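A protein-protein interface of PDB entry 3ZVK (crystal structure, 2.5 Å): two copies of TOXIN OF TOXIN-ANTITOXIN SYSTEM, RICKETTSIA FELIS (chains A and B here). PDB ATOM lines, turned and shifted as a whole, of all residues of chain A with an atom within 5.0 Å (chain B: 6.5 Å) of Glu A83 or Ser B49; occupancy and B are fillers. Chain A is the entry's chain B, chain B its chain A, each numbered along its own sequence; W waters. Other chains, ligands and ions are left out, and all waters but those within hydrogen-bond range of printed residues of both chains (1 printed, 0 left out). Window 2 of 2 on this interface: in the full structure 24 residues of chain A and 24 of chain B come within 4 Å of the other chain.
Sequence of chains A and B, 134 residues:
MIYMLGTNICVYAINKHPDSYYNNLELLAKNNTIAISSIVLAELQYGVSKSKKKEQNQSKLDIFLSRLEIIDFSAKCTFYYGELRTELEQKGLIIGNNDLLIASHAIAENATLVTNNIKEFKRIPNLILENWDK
Of the printed residues of chain B, Gly A82 touches Gln B45, Tyr B46 and Ser B49.
Of chain B, only Ser B49 (2.7 Å) comes within 4 Å of Glu A83.
Of the printed residues of chain B, Arg A85 touches Tyr B46 (3.3 Å).
Ser B49 touches just these residues of chain A: Gly A82 (3.3 Å), Glu A83 (2.7 Å) and Thr A86 (3.4 Å).
Printed residues of chain A within 4 Å of Lys B50: Thr A86.
The nearest residue of chain A that does not touch Ser B49 is Phe A79 (4.7 Å).
OG of Ser B49 is in hydrogen-bond range of OE2 of Glu A83 (2.7 Å).
The side-chain hydroxyl (OG1) of Thr A86 lies within hydrogen-bond range of the backbone NH (N) of Lys B50 (3.5 Å).
No position is printed for both chains.
Of the 9 pairs that touch across the chains among the printed residues, none has its exchanged pair printed and touching as well.
Water W1 lies within hydrogen-bond range of OG of Ser B49 (2.7 Å), NE2 of Gln B45 (2.9 Å) and O of Phe A79 (3.0 Å).
Along chain A the printed residues that touch a printed residue of chain B span positions 79 to 86.
Among the printed residues, 9 pairs touch across the chains.
Among the printed residues, merely in contact across the chains: Phe A79 with Gln B45 (3.998 Å), Gly A82 with Gln B45 (3.8 Å), Gly A82 with Tyr B46 (3.6 Å), Gly A82 with Ser B49 (3.3 Å), Arg A85 with Tyr B46 (3.3 Å), Thr A86 with Tyr B46 (3.7 Å) and Thr A86 with Ser B49 (3.4 Å).
The backbone carbonyl oxygen (O) of Gln B45 is in hydrogen-bond range of the side-chain hydroxyl (OG) of Ser B49 (3.3 Å).
OH of Tyr A81 lies within hydrogen-bond range of NH1 of Arg A85.
The backbone carbonyl oxygen (O) of Gly A82 lies within hydrogen-bond range of the side-chain hydroxyl (OG1) of Thr A86, 3.0 Å away.
NE2 of Gln B45 is in hydrogen-bond range of OE1 of Gln B58 (3.0 Å).
O of Ser B49 is in hydrogen-bond range of NZ of Lys B54, 2.8 Å away.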
ATOM      1  N   PHE A  79      14.218  26.028  10.998  1.00  0.00           N
ATOM      2  CA  PHE A  79      13.761  25.285   9.825  1.00  0.00           C
ATOM      3  C   PHE A  79      12.225  25.366   9.702  1.00  0.00           C
ATOM      4  O   PHE A  79      11.727  25.553   8.602  1.00  0.00           O
ATOM      5  CB  PHE A  79      14.231  23.817   9.862  1.00  0.00           C
ATOM      6  CG  PHE A  79      13.549  22.943   8.828  1.00  0.00           C
ATOM      7  CD1 PHE A  79      13.930  22.994   7.487  1.00  0.00           C
ATOM      8  CD2 PHE A  79      12.480  22.123   9.181  1.00  0.00           C
ATOM      9  CE1 PHE A  79      13.248  22.244   6.512  1.00  0.00           C
ATOM     10  CE2 PHE A  79      11.807  21.352   8.209  1.00  0.00           C
ATOM     11  CZ  PHE A  79      12.204  21.422   6.883  1.00  0.00           C
ATOM     12  N   TYR A  80      11.491  25.221  10.823  1.00  0.00           N
ATOM     13  CA  TYR A  80      10.034  25.276  10.885  1.00  0.00           C
ATOM     14  C   TYR A  80       9.542  26.661  10.549  1.00  0.00           C
ATOM     15  O   TYR A  80       8.577  26.779   9.811  1.00  0.00           O
ATOM     16  CB  TYR A  80       9.506  24.819  12.259  1.00  0.00           C
ATOM     17  CG  TYR A  80       9.925  23.413  12.585  1.00  0.00           C
ATOM     18  CD1 TYR A  80       9.296  22.324  11.996  1.00  0.00           C
ATOM     19  CD2 TYR A  80      11.023  23.167  13.405  1.00  0.00           C
ATOM     20  CE1 TYR A  80       9.726  21.023  12.246  1.00  0.00           C
ATOM     21  CE2 TYR A  80      11.461  21.872  13.661  1.00  0.00           C
ATOM     22  CZ  TYR A  80      10.811  20.803  13.082  1.00  0.00           C
ATOM     23  OH  TYR A  80      11.282  19.534  13.320  1.00  0.00           O
ATOM     24  N   TYR A  81      10.220  27.712  11.030  1.00  0.00           N
ATOM     25  CA  TYR A  81       9.857  29.102  10.723  1.00  0.00           C
ATOM     26  C   TYR A  81       9.981  29.348   9.202  1.00  0.00           C
ATOM     27  O   TYR A  81       9.100  29.967   8.607  1.00  0.00           O
ATOM     28  CB  TYR A  81      10.733  30.090  11.534  1.00  0.00           C
ATOM     29  CG  TYR A  81      10.628  31.526  11.071  1.00  0.00           C
ATOM     30  CD1 TYR A  81      11.478  32.026  10.081  1.00  0.00           C
ATOM     31  CD2 TYR A  81       9.713  32.395  11.641  1.00  0.00           C
ATOM     32  CE1 TYR A  81      11.392  33.344   9.652  1.00  0.00           C
ATOM     33  CE2 TYR A  81       9.630  33.727  11.230  1.00  0.00           C
ATOM     34  CZ  TYR A  81      10.473  34.195  10.239  1.00  0.00           C
ATOM     35  OH  TYR A  81      10.390  35.498   9.832  1.00  0.00           O
ATOM     36  N   GLY A  82      11.056  28.832   8.610  1.00  0.00           N
ATOM     37  CA  GLY A  82      11.318  28.968   7.184  1.00  0.00           C
ATOM     38  C   GLY A  82      10.231  28.378   6.316  1.00  0.00           C
ATOM     39  O   GLY A  82       9.750  29.013   5.382  1.00  0.00           O
ATOM     40  N   GLU A  83       9.809  27.185   6.675  1.00  0.00           N
ATOM     41  CA  GLU A  83       8.770  26.418   5.998  1.00  0.00           C
ATOM     42  C   GLU A  83       7.379  27.038   6.174  1.00  0.00           C
ATOM     43  O   GLU A  83       6.639  27.149   5.204  1.00  0.00           O
ATOM     44  CB  GLU A  83       8.799  24.955   6.474  1.00  0.00           C
ATOM     45  CG  GLU A  83      10.014  24.185   5.995  1.00  0.00           C
ATOM     46  CD  GLU A  83      10.012  23.833   4.518  1.00  0.00           C
ATOM     47  OE1 GLU A  83       9.339  22.847   4.150  1.00  0.00           O
ATOM     48  OE2 GLU A  83      10.705  24.522   3.732  1.00  0.00           O
ATOM     49  N   LEU A  84       7.048  27.458   7.411  1.00  0.00           N
ATOM     50  CA  LEU A  84       5.796  28.090   7.757  1.00  0.00           C
ATOM     51  C   LEU A  84       5.597  29.465   7.045  1.00  0.00           C
ATOM     52  O   LEU A  84       4.531  29.710   6.465  1.00  0.00           O
ATOM     53  CB  LEU A  84       5.663  28.203   9.285  1.00  0.00           C
ATOM     54  CG  LEU A  84       4.373  28.856   9.826  1.00  0.00           C
ATOM     55  CD1 LEU A  84       3.117  28.090   9.354  1.00  0.00           C
ATOM     56  CD2 LEU A  84       4.426  28.998  11.335  1.00  0.00           C
ATOM     57  N   ARG A  85       6.615  30.337   7.088  1.00  0.00           N
ATOM     58  CA  ARG A  85       6.566  31.651   6.464  1.00  0.00           C
ATOM     59  C   ARG A  85       6.327  31.543   4.951  1.00  0.00           C
ATOM     60  O   ARG A  85       5.461  32.252   4.409  1.00  0.00           O
ATOM     61  CB  ARG A  85       7.839  32.446   6.800  1.00  0.00           C
ATOM     62  CG  ARG A  85       7.750  33.899   6.329  1.00  0.00           C
ATOM     63  CD  ARG A  85       8.861  34.749   6.858  1.00  0.00           C
ATOM     64  NE  ARG A  85       8.948  36.000   6.112  1.00  0.00           N
ATOM     65  CZ  ARG A  85       9.918  36.888   6.271  1.00  0.00           C
ATOM     66  NH1 ARG A  85      10.894  36.660   7.135  1.00  0.00           N
ATOM     67  NH2 ARG A  85       9.959  37.981   5.518  1.00  0.00           N
ATOM     68  N   THR A  86       7.049  30.625   4.289  1.00  0.00           N
ATOM     69  CA  THR A  86       6.906  30.363   2.853  1.00  0.00           C
ATOM     70  C   THR A  86       5.502  29.905   2.503  1.00  0.00           C
ATOM     71  O   THR A  86       4.907  30.426   1.552  1.00  0.00           O
ATOM     72  CB  THR A  86       7.993  29.366   2.382  1.00  0.00           C
ATOM     73  OG1 THR A  86       9.251  29.987   2.622  1.00  0.00           O
ATOM     74  CG2 THR A  86       7.876  29.023   0.884  1.00  0.00           C
ATOM     75  N   GLU A  87       4.986  28.912   3.269  1.00  0.00           N
ATOM     76  CA  GLU A  87       3.674  28.319   3.059  1.00  0.00           C
ATOM     77  C   GLU A  87       2.561  29.343   3.253  1.00  0.00           C
ATOM     78  O   GLU A  87       1.668  29.401   2.432  1.00  0.00           O
ATOM     79  CB  GLU A  87       3.475  27.095   3.953  1.00  0.00           C
ATOM     80  CG  GLU A  87       2.254  26.270   3.558  1.00  0.00           C
ATOM     81  CD  GLU A  87       1.951  25.019   4.359  1.00  0.00           C
ATOM     82  OE1 GLU A  87       2.690  24.720   5.323  1.00  0.00           O
ATOM     83  OE2 GLU A  87       0.947  24.348   4.032  1.00  0.00           O
ATOM     84  N   LEU B  44      17.442  33.345   7.353  1.00  0.00           N
ATOM     85  CA  LEU B  44      18.221  32.582   6.369  1.00  0.00           C
ATOM     86  C   LEU B  44      17.504  31.279   5.966  1.00  0.00           C
ATOM     87  O   LEU B  44      17.451  30.937   4.789  1.00  0.00           O
ATOM     88  CB  LEU B  44      19.659  32.324   6.881  1.00  0.00           C
ATOM     89  CG  LEU B  44      20.546  33.558   7.138  1.00  0.00           C
ATOM     90  CD1 LEU B  44      21.841  33.126   7.785  1.00  0.00           C
ATOM     91  CD2 LEU B  44      20.793  34.408   5.844  1.00  0.00           C
ATOM     92  N   GLN B  45      16.891  30.589   6.936  1.00  0.00           N
ATOM     93  CA  GLN B  45      16.081  29.388   6.669  1.00  0.00           C
ATOM     94  C   GLN B  45      14.830  29.725   5.816  1.00  0.00           C
ATOM     95  O   GLN B  45      14.463  28.959   4.923  1.00  0.00           O
ATOM     96  CB  GLN B  45      15.711  28.666   7.969  1.00  0.00           C
ATOM     97  CG  GLN B  45      16.842  27.777   8.541  1.00  0.00           C
ATOM     98  CD  GLN B  45      17.256  26.614   7.645  1.00  0.00           C
ATOM     99  OE1 GLN B  45      18.359  26.138   7.714  1.00  0.00           O
ATOM    100  NE2 GLN B  45      16.407  26.156   6.735  1.00  0.00           N
ATOM    101  N   TYR B  46      14.236  30.899   6.034  1.00  0.00           N
ATOM    102  CA  TYR B  46      13.144  31.391   5.191  1.00  0.00           C
ATOM    103  C   TYR B  46      13.638  31.642   3.744  1.00  0.00           C
ATOM    104  O   TYR B  46      12.923  31.328   2.798  1.00  0.00           O
ATOM    105  CB  TYR B  46      12.496  32.659   5.795  1.00  0.00           C
ATOM    106  CG  TYR B  46      11.733  33.516   4.821  1.00  0.00           C
ATOM    107  CD1 TYR B  46      10.537  33.069   4.249  1.00  0.00           C
ATOM    108  CD2 TYR B  46      12.179  34.799   4.489  1.00  0.00           C
ATOM    109  CE1 TYR B  46       9.807  33.876   3.368  1.00  0.00           C
ATOM    110  CE2 TYR B  46      11.445  35.622   3.623  1.00  0.00           C
ATOM    111  CZ  TYR B  46      10.251  35.161   3.082  1.00  0.00           C
ATOM    112  OH  TYR B  46       9.518  35.969   2.239  1.00  0.00           O
ATOM    113  N   GLY B  47      14.851  32.180   3.603  1.00  0.00           N
ATOM    114  CA  GLY B  47      15.488  32.409   2.314  1.00  0.00           C
ATOM    115  C   GLY B  47      15.621  31.125   1.521  1.00  0.00           C
ATOM    116  O   GLY B  47      15.324  31.100   0.332  1.00  0.00           O
ATOM    117  N   VAL B  48      16.008  30.045   2.194  1.00  0.00           N
ATOM    118  CA  VAL B  48      16.175  28.702   1.620  1.00  0.00           C
ATOM    119  C   VAL B  48      14.832  28.123   1.174  1.00  0.00           C
ATOM    120  O   VAL B  48      14.697  27.701   0.026  1.00  0.00           O
ATOM    121  CB  VAL B  48      16.941  27.743   2.611  1.00  0.00           C
ATOM    122  CG1 VAL B  48      16.919  26.294   2.125  1.00  0.00           C
ATOM    123  CG2 VAL B  48      18.390  28.224   2.852  1.00  0.00           C
ATOM    124  N   SER B  49      13.847  28.101   2.077  1.00  0.00           N
ATOM    125  CA  SER B  49      12.513  27.534   1.814  1.00  0.00           C
ATOM    126  C   SER B  49      11.756  28.218   0.663  1.00  0.00           C
ATOM    127  O   SER B  49      10.997  27.568  -0.058  1.00  0.00           O
ATOM    128  CB  SER B  49      11.659  27.579   3.077  1.00  0.00           C
ATOM    129  OG  SER B  49      12.199  26.728   4.071  1.00  0.00           O
ATOM    130  N   LYS B  50      11.963  29.533   0.522  1.00  0.00           N
ATOM    131  CA  LYS B  50      11.334  30.391  -0.467  1.00  0.00           C
ATOM    132  C   LYS B  50      11.934  30.182  -1.874  1.00  0.00           C
ATOM    133  O   LYS B  50      11.202  30.257  -2.858  1.00  0.00           O
ATOM    134  CB  LYS B  50      11.501  31.848  -0.015  1.00  0.00           C
ATOM    135  CG  LYS B  50      10.863  32.849  -0.920  1.00  0.00           C
ATOM    136  CD  LYS B  50      10.471  34.081  -0.209  1.00  0.00           C
ATOM    137  CE  LYS B  50       9.677  34.897  -1.174  1.00  0.00           C
ATOM    138  NZ  LYS B  50       8.517  34.115  -1.639  1.00  0.00           N
ATOM    139  N   SER B  51      13.250  29.944  -1.957  1.00  0.00           N
ATOM    140  CA  SER B  51      14.022  29.790  -3.185  1.00  0.00           C
ATOM    141  C   SER B  51      13.621  28.611  -4.066  1.00  0.00           C
ATOM    142  O   SER B  51      12.879  27.719  -3.628  1.00  0.00           O
ATOM    143  CB  SER B  51      15.507  29.732  -2.856  1.00  0.00           C
ATOM    144  OG  SER B  51      15.879  28.478  -2.313  1.00  0.00           O
ATOM    145  N   LYS B  52      14.093  28.641  -5.332  1.00  0.00           N
ATOM    146  CA  LYS B  52      13.834  27.605  -6.340  1.00  0.00           C
ATOM    147  C   LYS B  52      14.812  26.432  -6.128  1.00  0.00           C
ATOM    148  O   LYS B  52      14.400  25.277  -6.168  1.00  0.00           O
ATOM    149  CB  LYS B  52      13.958  28.175  -7.774  1.00  0.00           C
ATOM    150  CG  LYS B  52      12.856  29.135  -8.181  1.00  0.00           C
ATOM    151  N   LYS B  54      16.372  24.901  -3.503  1.00  0.00           N
ATOM    152  CA  LYS B  54      16.318  24.620  -2.062  1.00  0.00           C
ATOM    153  C   LYS B  54      17.519  23.827  -1.514  1.00  0.00           C
ATOM    154  O   LYS B  54      18.127  24.257  -0.526  1.00  0.00           O
ATOM    155  CB  LYS B  54      14.985  23.980  -1.674  1.00  0.00           C
ATOM    156  CG  LYS B  54      13.786  24.919  -1.791  1.00  0.00           C
ATOM    157  CD  LYS B  54      12.520  24.310  -1.164  1.00  0.00           C
ATOM    158  CE  LYS B  54      11.287  24.463  -2.020  1.00  0.00           C
ATOM    159  NZ  LYS B  54      10.923  25.880  -2.302  1.00  0.00           N
ATOM    160  N   GLN B  58      20.410  25.331   0.860  1.00  0.00           N
ATOM    161  CA  GLN B  58      20.560  24.748   2.188  1.00  0.00           C
ATOM    162  C   GLN B  58      22.027  24.360   2.393  1.00  0.00           C
ATOM    163  O   GLN B  58      22.602  24.695   3.423  1.00  0.00           O
ATOM    164  CB  GLN B  58      19.627  23.550   2.388  1.00  0.00           C
ATOM    165  CG  GLN B  58      19.574  23.049   3.822  1.00  0.00           C
ATOM    166  CD  GLN B  58      19.084  24.058   4.833  1.00  0.00           C
ATOM    167  OE1 GLN B  58      17.932  24.444   4.839  1.00  0.00           O
ATOM    168  NE2 GLN B  58      19.906  24.421   5.785  1.00  0.00           N
HETATM  169  O   HOH W   1      13.522  26.389   6.398  1.00  0.00           O
